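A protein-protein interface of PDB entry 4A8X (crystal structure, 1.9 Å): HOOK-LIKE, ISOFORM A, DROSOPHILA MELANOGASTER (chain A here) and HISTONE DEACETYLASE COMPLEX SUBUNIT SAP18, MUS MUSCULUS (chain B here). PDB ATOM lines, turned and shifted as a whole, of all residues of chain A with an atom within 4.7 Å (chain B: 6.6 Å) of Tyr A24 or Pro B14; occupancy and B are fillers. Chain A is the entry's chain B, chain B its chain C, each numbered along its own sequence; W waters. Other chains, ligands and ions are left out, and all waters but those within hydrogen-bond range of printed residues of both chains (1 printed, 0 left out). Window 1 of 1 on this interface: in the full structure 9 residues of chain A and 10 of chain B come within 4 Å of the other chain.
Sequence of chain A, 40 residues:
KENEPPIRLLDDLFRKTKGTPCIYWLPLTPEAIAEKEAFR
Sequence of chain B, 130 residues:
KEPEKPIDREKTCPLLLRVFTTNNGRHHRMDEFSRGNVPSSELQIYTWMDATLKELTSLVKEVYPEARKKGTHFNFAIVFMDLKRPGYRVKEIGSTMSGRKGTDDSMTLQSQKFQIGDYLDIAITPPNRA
The side-chain sulfur (SG) of Cys B13 lies within hydrogen-bond range of the backbone carbonyl oxygen (O) of Tyr A24 (3.6 Å). The side-chain hydroxyl (OH) of Tyr B46 is in hydrogen-bond range of the backbone carbonyl oxygen (O) of Cys A22, at 2.5 Å.
The backbone carbonyl oxygen of Arg A15 is in hydrogen-bond range of the backbone NH of Trp A25, 2.8 Å away. The indole nitrogen of Trp B48 sits at hydrogen-bond distance from the backbone carbonyl oxygen of Thr B12, 2.9 Å away.
Leu A10 touches Trp B48 (CD2 to CH2, 3.99 Å). Phe A14 touches Arg B9. Thr B12 touches Phe A14. Cys B13 touches Phe A14 (CB to CD1, 3.3 Å). Phe A14 touches Pro B14 (CD2 to CD, 3.6 Å). OH of Tyr B46 touches CE of Lys A16 (3.9 Å). CD2 of Leu B16 touches O of Cys A22, 3.96 Å away. Tyr A24 touches Pro B14. CD1 of Tyr B46 touches CE2 of Tyr A24, 3.4 Å away. CA of Trp A25 touches SG of Cys B13, 3.9 Å away.
Of the printed residues of chain B, Phe A14 touches Arg B9 (3.5 Å), Thr B12 (3.3 Å), Cys B13 (3.3 Å) and Pro B14 (3.6 Å). Tyr A24 touches just these residues of chain B: Cys B13 (3.6 Å), Pro B14 (3.8 Å) and Tyr B46 (3.4 Å). Of the printed residues of chain B, Trp A25 touches Cys B13. Pro B14 touches two residues of chain A. Printed residues of chain A within 4 Å of Leu B16: Cys A22 (3.96 Å). Thr B47 touches none of the printed residues of chain A. The nearest residue of chain B that does not touch Tyr A24 is Leu B16 (6.2 Å).
Printed residues of chain A that touch a printed residue of chain B: Leu A10, Phe A14, Lys A16, Cys A22, Tyr A24 and Trp A25. Of the 9 printed residues of chain B, 7 touch a printed residue of chain A. Hydrophobic or aromatic side chains of chain B within 4 Å of the printed part of chain A: Pro B14, Leu B16, Tyr B46 and Trp B48. Among the printed residues, no Asp or Glu carboxylate lies within 4 Å of a Lys or Arg side-chain nitrogen of the other chain.
Water W1 lies within hydrogen-bond range of O of Pro B14, N of Tyr A24 and N of Leu B16.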
ATOM      1  N   LEU A  10      18.456 -32.688 -22.736  1.00  0.00           N
ATOM      2  CA  LEU A  10      17.568 -31.865 -23.578  1.00  0.00           C
ATOM      3  C   LEU A  10      16.147 -32.427 -23.614  1.00  0.00           C
ATOM      4  O   LEU A  10      15.168 -31.676 -23.547  1.00  0.00           O
ATOM      5  CB  LEU A  10      18.057 -31.738 -25.018  1.00  0.00           C
ATOM      6  CG  LEU A  10      19.319 -30.932 -25.305  1.00  0.00           C
ATOM      7  CD1 LEU A  10      19.458 -30.769 -26.821  1.00  0.00           C
ATOM      8  CD2 LEU A  10      19.282 -29.584 -24.597  1.00  0.00           C
ATOM      9  N   ASP A  11      16.038 -33.745 -23.715  1.00  0.00           N
ATOM     10  CA  ASP A  11      14.738 -34.391 -23.845  1.00  0.00           C
ATOM     11  C   ASP A  11      13.932 -34.387 -22.536  1.00  0.00           C
ATOM     12  O   ASP A  11      12.716 -34.529 -22.557  1.00  0.00           O
ATOM     13  CB  ASP A  11      14.927 -35.796 -24.416  1.00  0.00           C
ATOM     14  CG  ASP A  11      15.532 -35.760 -25.817  1.00  0.00           C
ATOM     15  OD1 ASP A  11      14.789 -35.413 -26.766  1.00  0.00           O
ATOM     16  OD2 ASP A  11      16.753 -36.029 -25.963  1.00  0.00           O
ATOM     17  N   PHE A  14      12.865 -30.170 -22.764  1.00  0.00           N
ATOM     18  CA  PHE A  14      12.186 -29.606 -23.908  1.00  0.00           C
ATOM     19  C   PHE A  14      11.474 -30.697 -24.699  1.00  0.00           C
ATOM     20  O   PHE A  14      11.859 -31.848 -24.618  1.00  0.00           O
ATOM     21  CB  PHE A  14      13.224 -28.919 -24.830  1.00  0.00           C
ATOM     22  CG  PHE A  14      14.095 -27.941 -24.092  1.00  0.00           C
ATOM     23  CD1 PHE A  14      13.540 -26.809 -23.525  1.00  0.00           C
ATOM     24  CD2 PHE A  14      15.441 -28.170 -23.936  1.00  0.00           C
ATOM     25  CE1 PHE A  14      14.312 -25.915 -22.830  1.00  0.00           C
ATOM     26  CE2 PHE A  14      16.222 -27.263 -23.253  1.00  0.00           C
ATOM     27  CZ  PHE A  14      15.660 -26.145 -22.695  1.00  0.00           C
ATOM     28  N   ARG A  15      10.462 -30.312 -25.477  1.00  0.00           N
ATOM     29  CA  ARG A  15       9.721 -31.241 -26.321  1.00  0.00           C
ATOM     30  C   ARG A  15      10.376 -31.321 -27.671  1.00  0.00           C
ATOM     31  O   ARG A  15      10.902 -30.347 -28.148  1.00  0.00           O
ATOM     32  CB  ARG A  15       8.276 -30.762 -26.454  1.00  0.00           C
ATOM     33  CG  ARG A  15       7.609 -30.678 -25.049  1.00  0.00           C
ATOM     34  CD  ARG A  15       6.121 -30.494 -25.098  1.00  0.00           C
ATOM     35  NE  ARG A  15       5.597 -30.298 -23.743  1.00  0.00           N
ATOM     36  CZ  ARG A  15       4.303 -30.284 -23.442  1.00  0.00           C
ATOM     37  NH1 ARG A  15       3.402 -30.446 -24.410  1.00  0.00           N
ATOM     38  NH2 ARG A  15       3.906 -30.104 -22.180  1.00  0.00           N
ATOM     39  N   LYS A  16      10.354 -32.483 -28.296  1.00  0.00           N
ATOM     40  CA  LYS A  16      11.004 -32.620 -29.594  1.00  0.00           C
ATOM     41  C   LYS A  16       9.996 -33.166 -30.594  1.00  0.00           C
ATOM     42  O   LYS A  16       9.253 -34.103 -30.277  1.00  0.00           O
ATOM     43  CB  LYS A  16      12.210 -33.543 -29.462  1.00  0.00           C
ATOM     44  CG  LYS A  16      13.072 -33.631 -30.676  1.00  0.00           C
ATOM     45  CD  LYS A  16      14.201 -34.634 -30.460  1.00  0.00           C
ATOM     46  CE  LYS A  16      15.228 -34.551 -31.614  1.00  0.00           C
ATOM     47  NZ  LYS A  16      16.350 -35.546 -31.568  1.00  0.00           N
ATOM     48  N   CYS A  22      14.181 -32.594 -37.010  1.00  0.00           N
ATOM     49  CA  CYS A  22      13.574 -32.509 -35.688  1.00  0.00           C
ATOM     50  C   CYS A  22      13.942 -31.183 -35.021  1.00  0.00           C
ATOM     51  O   CYS A  22      15.101 -30.765 -35.050  1.00  0.00           O
ATOM     52  CB  CYS A  22      14.008 -33.680 -34.812  1.00  0.00           C
ATOM     53  SG  CYS A  22      13.608 -35.265 -35.518  1.00  0.00           S
ATOM     54  N   ILE A  23      12.940 -30.534 -34.430  1.00  0.00           N
ATOM     55  CA  ILE A  23      13.139 -29.302 -33.702  1.00  0.00           C
ATOM     56  C   ILE A  23      12.589 -29.475 -32.308  1.00  0.00           C
ATOM     57  O   ILE A  23      11.736 -30.329 -32.063  1.00  0.00           O
ATOM     58  CB  ILE A  23      12.435 -28.081 -34.357  1.00  0.00           C
ATOM     59  CG1 ILE A  23      10.917 -28.309 -34.520  1.00  0.00           C
ATOM     60  CG2 ILE A  23      13.067 -27.792 -35.652  1.00  0.00           C
ATOM     61  CD1 ILE A  23      10.131 -27.097 -34.998  1.00  0.00           C
ATOM     62  N   TYR A  24      13.088 -28.660 -31.393  1.00  0.00           N
ATOM     63  CA  TYR A  24      12.566 -28.654 -30.038  1.00  0.00           C
ATOM     64  C   TYR A  24      11.540 -27.538 -29.895  1.00  0.00           C
ATOM     65  O   TYR A  24      11.547 -26.551 -30.660  1.00  0.00           O
ATOM     66  CB  TYR A  24      13.675 -28.491 -29.021  1.00  0.00           C
ATOM     67  CG  TYR A  24      14.546 -29.715 -28.861  1.00  0.00           C
ATOM     68  CD1 TYR A  24      14.241 -30.691 -27.933  1.00  0.00           C
ATOM     69  CD2 TYR A  24      15.673 -29.901 -29.658  1.00  0.00           C
ATOM     70  CE1 TYR A  24      15.029 -31.828 -27.790  1.00  0.00           C
ATOM     71  CE2 TYR A  24      16.453 -31.034 -29.548  1.00  0.00           C
ATOM     72  CZ  TYR A  24      16.145 -31.985 -28.590  1.00  0.00           C
ATOM     73  OH  TYR A  24      16.932 -33.090 -28.476  1.00  0.00           O
ATOM     74  N   TRP A  25      10.660 -27.686 -28.915  1.00  0.00           N
ATOM     75  CA  TRP A  25       9.681 -26.642 -28.591  1.00  0.00           C
ATOM     76  C   TRP A  25       9.256 -26.728 -27.137  1.00  0.00           C
ATOM     77  O   TRP A  25       9.540 -27.719 -26.453  1.00  0.00           O
ATOM     78  CB  TRP A  25       8.441 -26.743 -29.484  1.00  0.00           C
ATOM     79  CG  TRP A  25       7.593 -27.975 -29.333  1.00  0.00           C
ATOM     80  CD1 TRP A  25       7.848 -29.190 -29.835  1.00  0.00           C
ATOM     81  CD2 TRP A  25       6.311 -28.061 -28.681  1.00  0.00           C
ATOM     82  NE1 TRP A  25       6.815 -30.068 -29.530  1.00  0.00           N
ATOM     83  CE2 TRP A  25       5.858 -29.388 -28.821  1.00  0.00           C
ATOM     84  CE3 TRP A  25       5.507 -27.138 -27.997  1.00  0.00           C
ATOM     85  CZ2 TRP A  25       4.633 -29.824 -28.304  1.00  0.00           C
ATOM     86  CZ3 TRP A  25       4.285 -27.568 -27.476  1.00  0.00           C
ATOM     87  CH2 TRP A  25       3.869 -28.908 -27.629  1.00  0.00           C
ATOM     88  N   ARG B   9      20.060 -21.876 -20.592  1.00  0.00           N
ATOM     89  CA  ARG B   9      19.908 -23.034 -21.451  1.00  0.00           C
ATOM     90  C   ARG B   9      19.056 -24.167 -20.892  1.00  0.00           C
ATOM     91  O   ARG B   9      18.793 -25.144 -21.592  1.00  0.00           O
ATOM     92  CB  ARG B   9      21.281 -23.565 -21.853  1.00  0.00           C
ATOM     93  CG  ARG B   9      22.081 -22.566 -22.714  1.00  0.00           C
ATOM     94  CD  ARG B   9      23.464 -23.106 -23.099  1.00  0.00           C
ATOM     95  NE  ARG B   9      24.160 -22.193 -24.015  1.00  0.00           N
ATOM     96  CZ  ARG B   9      25.184 -22.544 -24.785  1.00  0.00           C
ATOM     97  NH1 ARG B   9      25.634 -23.780 -24.742  1.00  0.00           N
ATOM     98  NH2 ARG B   9      25.772 -21.651 -25.582  1.00  0.00           N
ATOM     99  N   THR B  12      15.429 -21.909 -22.033  1.00  0.00           N
ATOM    100  CA  THR B  12      15.272 -21.582 -23.453  1.00  0.00           C
ATOM    101  C   THR B  12      15.569 -22.804 -24.283  1.00  0.00           C
ATOM    102  O   THR B  12      16.637 -23.396 -24.161  1.00  0.00           O
ATOM    103  CB  THR B  12      16.233 -20.481 -23.857  1.00  0.00           C
ATOM    104  OG1 THR B  12      15.866 -19.280 -23.157  1.00  0.00           O
ATOM    105  CG2 THR B  12      16.192 -20.245 -25.395  1.00  0.00           C
ATOM    106  N   CYS B  13      14.628 -23.226 -25.118  1.00  0.00           N
ATOM    107  CA  CYS B  13      14.898 -24.431 -25.874  1.00  0.00           C
ATOM    108  C   CYS B  13      15.918 -24.135 -27.000  1.00  0.00           C
ATOM    109  O   CYS B  13      16.042 -23.018 -27.478  1.00  0.00           O
ATOM    110  CB  CYS B  13      13.615 -25.144 -26.325  1.00  0.00           C
ATOM    111  SG  CYS B  13      12.964 -24.731 -27.936  1.00  0.00           S
ATOM    112  N   PRO B  14      16.721 -25.129 -27.340  1.00  0.00           N
ATOM    113  CA  PRO B  14      17.761 -24.896 -28.341  1.00  0.00           C
ATOM    114  C   PRO B  14      17.211 -24.787 -29.757  1.00  0.00           C
ATOM    115  O   PRO B  14      16.144 -25.317 -30.022  1.00  0.00           O
ATOM    116  CB  PRO B  14      18.605 -26.151 -28.239  1.00  0.00           C
ATOM    117  CG  PRO B  14      17.648 -27.206 -27.843  1.00  0.00           C
ATOM    118  CD  PRO B  14      16.712 -26.513 -26.871  1.00  0.00           C
ATOM    119  N   LEU B  15      17.996 -24.180 -30.650  1.00  0.00           N
ATOM    120  CA  LEU B  15      17.659 -24.038 -32.055  1.00  0.00           C
ATOM    121  C   LEU B  15      18.386 -25.121 -32.802  1.00  0.00           C
ATOM    122  O   LEU B  15      19.458 -25.581 -32.350  1.00  0.00           O
ATOM    123  CB  LEU B  15      18.111 -22.643 -32.579  1.00  0.00           C
ATOM    124  CG  LEU B  15      19.613 -22.341 -32.537  1.00  0.00           C
ATOM    125  CD1 LEU B  15      20.276 -22.456 -33.902  1.00  0.00           C
ATOM    126  CD2 LEU B  15      19.906 -20.965 -31.901  1.00  0.00           C
ATOM    127  N   LEU B  16      17.794 -25.544 -33.919  1.00  0.00           N
ATOM    128  CA  LEU B  16      18.417 -26.506 -34.814  1.00  0.00           C
ATOM    129  C   LEU B  16      19.380 -25.742 -35.733  1.00  0.00           C
ATOM    130  O   LEU B  16      18.964 -24.825 -36.441  1.00  0.00           O
ATOM    131  CB  LEU B  16      17.388 -27.181 -35.710  1.00  0.00           C
ATOM    132  CG  LEU B  16      17.974 -28.037 -36.859  1.00  0.00           C
ATOM    133  CD1 LEU B  16      18.740 -29.220 -36.337  1.00  0.00           C
ATOM    134  CD2 LEU B  16      16.846 -28.494 -37.782  1.00  0.00           C
ATOM    135  N   TYR B  46      22.236 -28.879 -31.999  1.00  0.00           N
ATOM    136  CA  TYR B  46      21.239 -28.126 -31.260  1.00  0.00           C
ATOM    137  C   TYR B  46      21.960 -27.157 -30.340  1.00  0.00           C
ATOM    138  O   TYR B  46      22.707 -27.576 -29.441  1.00  0.00           O
ATOM    139  CB  TYR B  46      20.328 -29.085 -30.473  1.00  0.00           C
ATOM    140  CG  TYR B  46      19.433 -29.868 -31.399  1.00  0.00           C
ATOM    141  CD1 TYR B  46      18.277 -29.310 -31.915  1.00  0.00           C
ATOM    142  CD2 TYR B  46      19.788 -31.161 -31.820  1.00  0.00           C
ATOM    143  CE1 TYR B  46      17.487 -30.003 -32.758  1.00  0.00           C
ATOM    144  CE2 TYR B  46      19.001 -31.860 -32.678  1.00  0.00           C
ATOM    145  CZ  TYR B  46      17.846 -31.292 -33.156  1.00  0.00           C
ATOM    146  OH  TYR B  46      17.048 -32.022 -34.034  1.00  0.00           O
ATOM    147  N   THR B  47      21.733 -25.869 -30.531  1.00  0.00           N
ATOM    148  CA  THR B  47      22.511 -24.883 -29.788  1.00  0.00           C
ATOM    149  C   THR B  47      21.675 -23.646 -29.435  1.00  0.00           C
ATOM    150  O   THR B  47      20.425 -23.692 -29.450  1.00  0.00           O
ATOM    151  CB  THR B  47      23.853 -24.542 -30.585  1.00  0.00           C
ATOM    152  OG1 THR B  47      24.739 -23.762 -29.775  1.00  0.00           O
ATOM    153  CG2 THR B  47      23.570 -23.794 -31.858  1.00  0.00           C
ATOM    154  N   TRP B  48      22.358 -22.559 -29.086  1.00  0.00           N
ATOM    155  CA  TRP B  48      21.728 -21.359 -28.573  1.00  0.00           C
ATOM    156  C   TRP B  48      22.367 -20.147 -29.237  1.00  0.00           C
ATOM    157  O   TRP B  48      23.466 -20.245 -29.757  1.00  0.00           O
ATOM    158  CB  TRP B  48      21.883 -21.277 -27.040  1.00  0.00           C
ATOM    159  CG  TRP B  48      21.048 -22.294 -26.318  1.00  0.00           C
ATOM    160  CD1 TRP B  48      19.771 -22.117 -25.816  1.00  0.00           C
ATOM    161  CD2 TRP B  48      21.412 -23.639 -26.011  1.00  0.00           C
ATOM    162  NE1 TRP B  48      19.331 -23.277 -25.243  1.00  0.00           N
ATOM    163  CE2 TRP B  48      20.319 -24.226 -25.336  1.00  0.00           C
ATOM    164  CE3 TRP B  48      22.560 -24.412 -26.235  1.00  0.00           C
ATOM    165  CZ2 TRP B  48      20.344 -25.556 -24.879  1.00  0.00           C
ATOM    166  CZ3 TRP B  48      22.566 -25.744 -25.805  1.00  0.00           C
ATOM    167  CH2 TRP B  48      21.472 -26.294 -25.129  1.00  0.00           C
HETATM  168  O   HOH W   1      15.084 -26.719 -32.201  1.00  0.00           O
